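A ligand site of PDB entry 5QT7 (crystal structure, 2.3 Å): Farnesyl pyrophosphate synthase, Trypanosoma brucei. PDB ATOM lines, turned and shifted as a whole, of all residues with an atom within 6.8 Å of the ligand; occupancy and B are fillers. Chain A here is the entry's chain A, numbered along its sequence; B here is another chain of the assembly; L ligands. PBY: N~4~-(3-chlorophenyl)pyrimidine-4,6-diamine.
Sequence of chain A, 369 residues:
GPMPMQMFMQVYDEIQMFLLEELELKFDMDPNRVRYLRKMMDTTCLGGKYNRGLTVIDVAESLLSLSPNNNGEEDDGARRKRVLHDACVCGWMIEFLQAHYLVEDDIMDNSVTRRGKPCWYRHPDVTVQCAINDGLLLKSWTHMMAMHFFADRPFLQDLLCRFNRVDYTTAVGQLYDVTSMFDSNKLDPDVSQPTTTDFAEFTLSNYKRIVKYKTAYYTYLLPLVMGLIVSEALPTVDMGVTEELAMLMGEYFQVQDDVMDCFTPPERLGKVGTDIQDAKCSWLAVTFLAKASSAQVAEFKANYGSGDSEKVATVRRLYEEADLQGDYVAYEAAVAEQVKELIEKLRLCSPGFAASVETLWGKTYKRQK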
ATOM      1  N   ARG A  52       5.642  32.926 -21.071  1.00  0.00           N
ATOM      2  CA  ARG A  52       6.171  33.164 -22.407  1.00  0.00           C
ATOM      3  C   ARG A  52       5.498  34.371 -23.056  1.00  0.00           C
ATOM      4  O   ARG A  52       6.172  35.210 -23.678  1.00  0.00           O
ATOM      5  CB  ARG A  52       5.983  31.917 -23.277  1.00  0.00           C
ATOM      6  CG  ARG A  52       6.691  30.692 -22.733  1.00  0.00           C
ATOM      7  CD  ARG A  52       6.247  29.431 -23.458  1.00  0.00           C
ATOM      8  NE  ARG A  52       6.847  28.233 -22.873  1.00  0.00           N
ATOM      9  CZ  ARG A  52       6.384  27.627 -21.780  1.00  0.00           C
ATOM     10  NH1 ARG A  52       5.328  28.109 -21.150  1.00  0.00           N
ATOM     11  NH2 ARG A  52       6.990  26.544 -21.320  1.00  0.00           N
ATOM     12  N   GLN A  98       1.613  26.881 -26.665  1.00  0.00           N
ATOM     13  CA  GLN A  98       1.795  26.079 -25.468  1.00  0.00           C
ATOM     14  C   GLN A  98       0.542  25.264 -25.161  1.00  0.00           C
ATOM     15  O   GLN A  98       0.626  24.098 -24.766  1.00  0.00           O
ATOM     16  CB  GLN A  98       2.157  26.962 -24.280  1.00  0.00           C
ATOM     17  CG  GLN A  98       2.245  26.232 -22.946  1.00  0.00           C
ATOM     18  CD  GLN A  98       3.431  25.288 -22.839  1.00  0.00           C
ATOM     19  OE1 GLN A  98       4.271  25.227 -23.741  1.00  0.00           O
ATOM     20  NE2 GLN A  98       3.506  24.545 -21.742  1.00  0.00           N
ATOM     21  N   HIS A 100      -1.469  24.189 -27.418  1.00  0.00           N
ATOM     22  CA  HIS A 100      -1.388  23.106 -28.389  1.00  0.00           C
ATOM     23  C   HIS A 100      -0.490  21.981 -27.894  1.00  0.00           C
ATOM     24  O   HIS A 100      -0.824  20.800 -28.035  1.00  0.00           O
ATOM     25  CB  HIS A 100      -0.876  23.648 -29.726  1.00  0.00           C
ATOM     26  CG  HIS A 100      -0.301  22.593 -30.635  1.00  0.00           C
ATOM     27  ND1 HIS A 100      -1.064  21.590 -31.192  1.00  0.00           N
ATOM     28  CD2 HIS A 100       0.958  22.396 -31.080  1.00  0.00           C
ATOM     29  CE1 HIS A 100      -0.297  20.821 -31.942  1.00  0.00           C
ATOM     30  NE2 HIS A 100       0.937  21.289 -31.893  1.00  0.00           N
ATOM     31  N   TYR A 101       0.661  22.329 -27.293  1.00  0.00           N
ATOM     32  CA  TYR A 101       1.547  21.306 -26.762  1.00  0.00           C
ATOM     33  C   TYR A 101       0.931  20.589 -25.577  1.00  0.00           C
ATOM     34  O   TYR A 101       1.093  19.370 -25.415  1.00  0.00           O
ATOM     35  CB  TYR A 101       2.889  21.927 -26.364  1.00  0.00           C
ATOM     36  CG  TYR A 101       3.737  22.398 -27.533  1.00  0.00           C
ATOM     37  CD1 TYR A 101       3.492  21.932 -28.821  1.00  0.00           C
ATOM     38  CD2 TYR A 101       4.767  23.296 -27.337  1.00  0.00           C
ATOM     39  CE1 TYR A 101       4.267  22.359 -29.888  1.00  0.00           C
ATOM     40  CE2 TYR A 101       5.549  23.728 -28.392  1.00  0.00           C
ATOM     41  CZ  TYR A 101       5.299  23.259 -29.667  1.00  0.00           C
ATOM     42  OH  TYR A 101       6.068  23.684 -30.721  1.00  0.00           O
ATOM     43  N   LEU A 102       0.200  21.325 -24.728  1.00  0.00           N
ATOM     44  CA  LEU A 102      -0.430  20.699 -23.563  1.00  0.00           C
ATOM     45  C   LEU A 102      -1.505  19.703 -23.992  1.00  0.00           C
ATOM     46  O   LEU A 102      -1.662  18.650 -23.364  1.00  0.00           O
ATOM     47  CB  LEU A 102      -1.028  21.768 -22.646  1.00  0.00           C
ATOM     48  CG  LEU A 102      -0.039  22.702 -21.939  1.00  0.00           C
ATOM     49  CD1 LEU A 102      -0.794  23.666 -21.037  1.00  0.00           C
ATOM     50  CD2 LEU A 102       0.982  21.903 -21.143  1.00  0.00           C
ATOM     51  N   GLU A 104      -1.530  17.997 -26.837  1.00  0.00           N
ATOM     52  CA  GLU A 104      -0.817  16.834 -27.359  1.00  0.00           C
ATOM     53  C   GLU A 104      -0.297  15.950 -26.240  1.00  0.00           C
ATOM     54  O   GLU A 104      -0.175  14.723 -26.415  1.00  0.00           O
ATOM     55  CB  GLU A 104       0.327  17.276 -28.260  1.00  0.00           C
ATOM     56  CG  GLU A 104      -0.095  18.037 -29.517  1.00  0.00           C
ATOM     57  CD  GLU A 104      -0.989  17.214 -30.422  1.00  0.00           C
ATOM     58  OE1 GLU A 104      -1.929  17.783 -31.011  1.00  0.00           O
ATOM     59  OE2 GLU A 104      -0.742  15.995 -30.556  1.00  0.00           O
ATOM     60  N   ASP A 105       0.031  16.524 -25.086  1.00  0.00           N
ATOM     61  CA  ASP A 105       0.494  15.727 -23.958  1.00  0.00           C
ATOM     62  C   ASP A 105      -0.653  14.922 -23.348  1.00  0.00           C
ATOM     63  O   ASP A 105      -0.449  13.773 -22.921  1.00  0.00           O
ATOM     64  CB  ASP A 105       1.136  16.619 -22.891  1.00  0.00           C
ATOM     65  CG  ASP A 105       2.374  17.335 -23.397  1.00  0.00           C
ATOM     66  OD1 ASP A 105       2.978  16.847 -24.376  1.00  0.00           O
ATOM     67  OD2 ASP A 105       2.737  18.368 -22.818  1.00  0.00           O
ATOM     68  N   MET A 108      -1.146  11.686 -25.242  1.00  0.00           N
ATOM     69  CA  MET A 108      -0.154  10.650 -24.980  1.00  0.00           C
ATOM     70  C   MET A 108      -0.500   9.832 -23.748  1.00  0.00           C
ATOM     71  O   MET A 108      -0.127   8.657 -23.651  1.00  0.00           O
ATOM     72  CB  MET A 108       1.234  11.266 -24.833  1.00  0.00           C
ATOM     73  CG  MET A 108       1.829  11.783 -26.144  1.00  0.00           C
ATOM     74  SD  MET A 108       3.416  12.610 -25.947  1.00  0.00           S
ATOM     75  CE  MET A 108       3.861  12.894 -27.660  1.00  0.00           C
ATOM     76  N   ASP A 167       8.617  25.728 -33.790  1.00  0.00           N
ATOM     77  CA  ASP A 167       7.679  24.644 -33.555  1.00  0.00           C
ATOM     78  C   ASP A 167       8.212  23.330 -34.102  1.00  0.00           C
ATOM     79  O   ASP A 167       8.064  22.275 -33.470  1.00  0.00           O
ATOM     80  CB  ASP A 167       6.319  24.989 -34.180  1.00  0.00           C
ATOM     81  CG  ASP A 167       5.326  23.860 -34.079  1.00  0.00           C
ATOM     82  OD1 ASP A 167       4.924  23.518 -32.949  1.00  0.00           O
ATOM     83  OD2 ASP A 167       4.945  23.307 -35.135  1.00  0.00           O
ATOM     84  N   THR A 170      10.822  22.186 -31.623  1.00  0.00           N
ATOM     85  CA  THR A 170      10.267  21.552 -30.432  1.00  0.00           C
ATOM     86  C   THR A 170       9.873  20.109 -30.701  1.00  0.00           C
ATOM     87  O   THR A 170      10.072  19.226 -29.848  1.00  0.00           O
ATOM     88  CB  THR A 170       9.065  22.345 -29.919  1.00  0.00           C
ATOM     89  OG1 THR A 170       9.424  23.732 -29.810  1.00  0.00           O
ATOM     90  CG2 THR A 170       8.645  21.837 -28.556  1.00  0.00           C
ATOM     91  N   ALA A 171       9.314  19.834 -31.885  1.00  0.00           N
ATOM     92  CA  ALA A 171       8.950  18.466 -32.214  1.00  0.00           C
ATOM     93  C   ALA A 171      10.180  17.580 -32.357  1.00  0.00           C
ATOM     94  O   ALA A 171      10.172  16.423 -31.942  1.00  0.00           O
ATOM     95  CB  ALA A 171       8.115  18.446 -33.498  1.00  0.00           C
ATOM     96  N   VAL A 172      11.249  18.121 -32.956  1.00  0.00           N
ATOM     97  CA  VAL A 172      12.516  17.382 -33.006  1.00  0.00           C
ATOM     98  C   VAL A 172      13.053  17.169 -31.592  1.00  0.00           C
ATOM     99  O   VAL A 172      13.585  16.104 -31.279  1.00  0.00           O
ATOM    100  CB  VAL A 172      13.523  18.125 -33.901  1.00  0.00           C
ATOM    101  CG1 VAL A 172      14.885  17.453 -33.835  1.00  0.00           C
ATOM    102  CG2 VAL A 172      13.030  18.182 -35.341  1.00  0.00           C
ATOM    103  N   GLN A 174      11.291  16.816 -28.881  1.00  0.00           N
ATOM    104  CA  GLN A 174      10.505  15.781 -28.220  1.00  0.00           C
ATOM    105  C   GLN A 174      10.924  14.385 -28.686  1.00  0.00           C
ATOM    106  O   GLN A 174      10.787  13.416 -27.937  1.00  0.00           O
ATOM    107  CB  GLN A 174       9.014  15.996 -28.465  1.00  0.00           C
ATOM    108  CG  GLN A 174       8.115  15.349 -27.421  1.00  0.00           C
ATOM    109  CD  GLN A 174       8.312  15.953 -26.044  1.00  0.00           C
ATOM    110  OE1 GLN A 174       8.553  17.153 -25.904  1.00  0.00           O
ATOM    111  NE2 GLN A 174       8.218  15.116 -25.011  1.00  0.00           N
ATOM    112  N   LEU A 175      11.438  14.273 -29.919  1.00  0.00           N
ATOM    113  CA  LEU A 175      11.927  12.983 -30.394  1.00  0.00           C
ATOM    114  C   LEU A 175      13.201  12.573 -29.668  1.00  0.00           C
ATOM    115  O   LEU A 175      13.403  11.391 -29.369  1.00  0.00           O
ATOM    116  CB  LEU A 175      12.153  13.044 -31.898  1.00  0.00           C
ATOM    117  CG  LEU A 175      12.852  11.852 -32.569  1.00  0.00           C
ATOM    118  CD1 LEU A 175      12.052  10.573 -32.367  1.00  0.00           C
ATOM    119  CD2 LEU A 175      13.060  12.125 -34.044  1.00  0.00           C
ATOM    120  N   VAL A 178      11.929  11.535 -26.045  1.00  0.00           N
ATOM    121  CA  VAL A 178      11.158  10.299 -25.971  1.00  0.00           C
ATOM    122  C   VAL A 178      12.046   9.091 -26.221  1.00  0.00           C
ATOM    123  O   VAL A 178      11.911   8.052 -25.559  1.00  0.00           O
ATOM    124  CB  VAL A 178       9.973  10.366 -26.967  1.00  0.00           C
ATOM    125  CG1 VAL A 178       9.464   8.968 -27.287  1.00  0.00           C
ATOM    126  CG2 VAL A 178       8.854  11.216 -26.398  1.00  0.00           C
ATOM    127  N   LYS A 214      13.922  20.797 -27.041  1.00  0.00           N
ATOM    128  CA  LYS A 214      12.618  20.507 -26.450  1.00  0.00           C
ATOM    129  C   LYS A 214      12.063  21.713 -25.700  1.00  0.00           C
ATOM    130  O   LYS A 214      10.853  21.948 -25.705  1.00  0.00           O
ATOM    131  CB  LYS A 214      12.698  19.306 -25.520  1.00  0.00           C
ATOM    132  CG  LYS A 214      11.334  18.794 -25.073  1.00  0.00           C
ATOM    133  CD  LYS A 214      11.422  17.802 -23.913  1.00  0.00           C
ATOM    134  CE  LYS A 214      11.627  18.508 -22.585  1.00  0.00           C
ATOM    135  NZ  LYS A 214      11.138  17.690 -21.430  1.00  0.00           N
ATOM    136  N   THR A 215      12.931  22.474 -25.037  1.00  0.00           N
ATOM    137  CA  THR A 215      12.501  23.564 -24.167  1.00  0.00           C
ATOM    138  C   THR A 215      13.071  24.921 -24.565  1.00  0.00           C
ATOM    139  O   THR A 215      12.318  25.887 -24.711  1.00  0.00           O
ATOM    140  CB  THR A 215      12.881  23.250 -22.706  1.00  0.00           C
ATOM    141  OG1 THR A 215      12.213  22.059 -22.279  1.00  0.00           O
ATOM    142  CG2 THR A 215      12.506  24.401 -21.789  1.00  0.00           C
ATOM    143  N   TYR A 218      11.623  27.421 -27.754  1.00  0.00           N
ATOM    144  CA  TYR A 218      10.291  28.000 -27.755  1.00  0.00           C
ATOM    145  C   TYR A 218       9.894  28.612 -26.417  1.00  0.00           C
ATOM    146  O   TYR A 218       8.916  29.365 -26.362  1.00  0.00           O
ATOM    147  CB  TYR A 218       9.255  26.941 -28.164  1.00  0.00           C
ATOM    148  CG  TYR A 218       8.578  26.220 -27.018  1.00  0.00           C
ATOM    149  CD1 TYR A 218       9.219  25.190 -26.344  1.00  0.00           C
ATOM    150  CD2 TYR A 218       7.282  26.552 -26.634  1.00  0.00           C
ATOM    151  CE1 TYR A 218       8.607  24.529 -25.302  1.00  0.00           C
ATOM    152  CE2 TYR A 218       6.663  25.886 -25.603  1.00  0.00           C
ATOM    153  CZ  TYR A 218       7.322  24.879 -24.941  1.00  0.00           C
ATOM    154  OH  TYR A 218       6.691  24.220 -23.905  1.00  0.00           O
ATOM    155  N   THR A 219      10.646  28.346 -25.351  1.00  0.00           N
ATOM    156  CA  THR A 219      10.317  28.916 -24.040  1.00  0.00           C
ATOM    157  C   THR A 219      11.091  30.211 -23.774  1.00  0.00           C
ATOM    158  O   THR A 219      10.551  31.138 -23.157  1.00  0.00           O
ATOM    159  CB  THR A 219      10.602  27.895 -22.933  1.00  0.00           C
ATOM    160  OG1 THR A 219       9.874  26.694 -23.204  1.00  0.00           O
ATOM    161  CG2 THR A 219      10.171  28.442 -21.581  1.00  0.00           C
ATOM    162  N   GLN B 129       3.638   7.828 -28.435  1.00  0.00           N
ATOM    163  CA  GLN B 129       4.395   9.074 -28.406  1.00  0.00           C
ATOM    164  C   GLN B 129       5.032   9.360 -29.762  1.00  0.00           C
ATOM    165  O   GLN B 129       5.034  10.499 -30.229  1.00  0.00           O
ATOM    166  CB  GLN B 129       5.473   9.003 -27.322  1.00  0.00           C
ATOM    167  CG  GLN B 129       4.928   8.840 -25.917  1.00  0.00           C
ATOM    168  CD  GLN B 129       6.001   8.421 -24.932  1.00  0.00           C
ATOM    169  OE1 GLN B 129       7.100   8.028 -25.324  1.00  0.00           O
ATOM    170  NE2 GLN B 129       5.677   8.486 -23.650  1.00  0.00           N
ATOM    171  N   ILE B 132       2.259  10.428 -32.408  1.00  0.00           N
ATOM    172  CA  ILE B 132       1.877  11.825 -32.226  1.00  0.00           C
ATOM    173  C   ILE B 132       2.984  12.747 -32.716  1.00  0.00           C
ATOM    174  O   ILE B 132       2.735  13.750 -33.391  1.00  0.00           O
ATOM    175  CB  ILE B 132       1.519  12.086 -30.756  1.00  0.00           C
ATOM    176  CG1 ILE B 132       0.240  11.333 -30.387  1.00  0.00           C
ATOM    177  CG2 ILE B 132       1.366  13.579 -30.494  1.00  0.00           C
ATOM    178  CD1 ILE B 132      -0.268  11.623 -28.992  1.00  0.00           C
ATOM    179  N   ASN B 133       4.241  12.414 -32.395  1.00  0.00           N
ATOM    180  CA  ASN B 133       5.362  13.239 -32.835  1.00  0.00           C
ATOM    181  C   ASN B 133       5.533  13.162 -34.352  1.00  0.00           C
ATOM    182  O   ASN B 133       5.860  14.172 -34.992  1.00  0.00           O
ATOM    183  CB  ASN B 133       6.637  12.824 -32.117  1.00  0.00           C
ATOM    184  CG  ASN B 133       7.854  13.604 -32.573  1.00  0.00           C
ATOM    185  OD1 ASN B 133       8.714  13.083 -33.292  1.00  0.00           O
ATOM    186  ND2 ASN B 133       7.931  14.863 -32.164  1.00  0.00           N
ATOM    187  N   ASP B 134       5.327  11.979 -34.943  1.00  0.00           N
ATOM    188  CA  ASP B 134       5.458  11.848 -36.393  1.00  0.00           C
ATOM    189  C   ASP B 134       4.405  12.678 -37.118  1.00  0.00           C
ATOM    190  O   ASP B 134       4.681  13.245 -38.181  1.00  0.00           O
ATOM    191  CB  ASP B 134       5.368  10.380 -36.803  1.00  0.00           C
ATOM    192  CG  ASP B 134       6.591   9.586 -36.390  1.00  0.00           C
ATOM    193  OD1 ASP B 134       7.662  10.194 -36.196  1.00  0.00           O
ATOM    194  OD2 ASP B 134       6.478   8.345 -36.274  1.00  0.00           O
ATOM    195  N   LEU B 136       3.148  15.533 -36.103  1.00  0.00           N
ATOM    196  CA  LEU B 136       3.567  16.933 -36.039  1.00  0.00           C
ATOM    197  C   LEU B 136       4.760  17.202 -36.950  1.00  0.00           C
ATOM    198  O   LEU B 136       4.883  18.293 -37.501  1.00  0.00           O
ATOM    199  CB  LEU B 136       3.890  17.332 -34.602  1.00  0.00           C
ATOM    200  CG  LEU B 136       2.743  17.268 -33.600  1.00  0.00           C
ATOM    201  CD1 LEU B 136       3.187  17.792 -32.250  1.00  0.00           C
ATOM    202  CD2 LEU B 136       1.530  18.050 -34.104  1.00  0.00           C
HETATM  203  C2  PBY L   1       5.171  18.654 -27.275  1.00  0.00           C
HETATM  204  C3  PBY L   1       5.620  19.603 -25.117  1.00  0.00           C
HETATM  205  C11 PBY L   1       7.660  20.656 -24.558  1.00  0.00           C
HETATM  206  C12 PBY L   1       5.818  18.020 -29.946  1.00  0.00           C
HETATM  207  C10 PBY L   1       5.946  20.628 -22.946  1.00  0.00           C
HETATM  208  C4  PBY L   1       4.917  17.374 -27.793  1.00  0.00           C
HETATM  209  C5  PBY L   1       5.750  19.613 -28.127  1.00  0.00           C
HETATM  210  C6  PBY L   1       5.129  19.931 -23.847  1.00  0.00           C
HETATM  211  C8  PBY L   1       5.235  17.064 -29.110  1.00  0.00           C
HETATM  212  C9  PBY L   1       6.079  19.296 -29.449  1.00  0.00           C
HETATM  213  N1  PBY L   1       4.837  18.927 -25.986  1.00  0.00           N
HETATM  214  N14 PBY L   1       7.192  20.975 -23.327  1.00  0.00           N
HETATM  215  N15 PBY L   1       5.512  20.960 -21.716  1.00  0.00           N
HETATM  216  N7  PBY L   1       6.877  19.980 -25.428  1.00  0.00           N
HETATM  217 CL13 PBY L   1       4.916  15.454 -29.731  1.00  0.00          CL
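A nitrogen (N14) of the ligand is in hydrogen-bond range of the side-chain hydroxyl (OH) of Tyr 218 (3.3 Å).
The side-chain amide oxygen (OE1) of Gln 174 sits close to a nitrogen (N7) of the ligand (3.3 Å).
N1 of the ligand lies within hydrogen-bond range of OD1 of Asp 105 (3.2 Å).
Tyr 101 touches the ligand (CD1 to C5, 3.3 Å).
Met 108 touches the ligand (CE to CL13, 3.5 Å).
Thr 170 touches the ligand (CG2 to C5, 3.7 Å).
Ala 171 touches the ligand (CA to C12, 3.9 Å).
O of Lys 214 touches C11 of the ligand (3.6 Å).
CA of Asn 133 of chain B touches CL13 of the ligand (3.8 Å).
Leu 136 of chain B touches the ligand.
Hydrophobic or aromatic side chains within 4 Å of the ligand: Tyr 101, Met 108 and Leu 136 of chain B.
Within 4 Å of the ligand: Tyr 101, Asp 105, Met 108, Thr 170, Ala 171, Gln 174, Lys 214, Tyr 218, Asn 133 of chain B and Leu 136 of chain B.
The nearest printed residue that does not touch the ligand is Ile 132 of chain B (4.1 Å).
The side-chain hydroxyl (OH) of Tyr 218 lies within hydrogen-bond range of the side-chain amide oxygen (OE1) of Gln 98, 2.6 Å away.
The side-chain hydroxyl (OH) of Tyr 218 lies within hydrogen-bond range of the guanidinium group (NH2) of Arg 52.
The side-chain hydroxyl of Tyr 101 sits at hydrogen-bond distance from the side-chain carboxylate of Asp 167, at 2.5 Å.
The backbone carbonyl oxygen of Ala 171 sits at hydrogen-bond distance from the side-chain amide nitrogen of Asn 133 of chain B (2.7 Å).
OG1 of Thr 170 sits close to OH of Tyr 101, 3.5 Å away.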
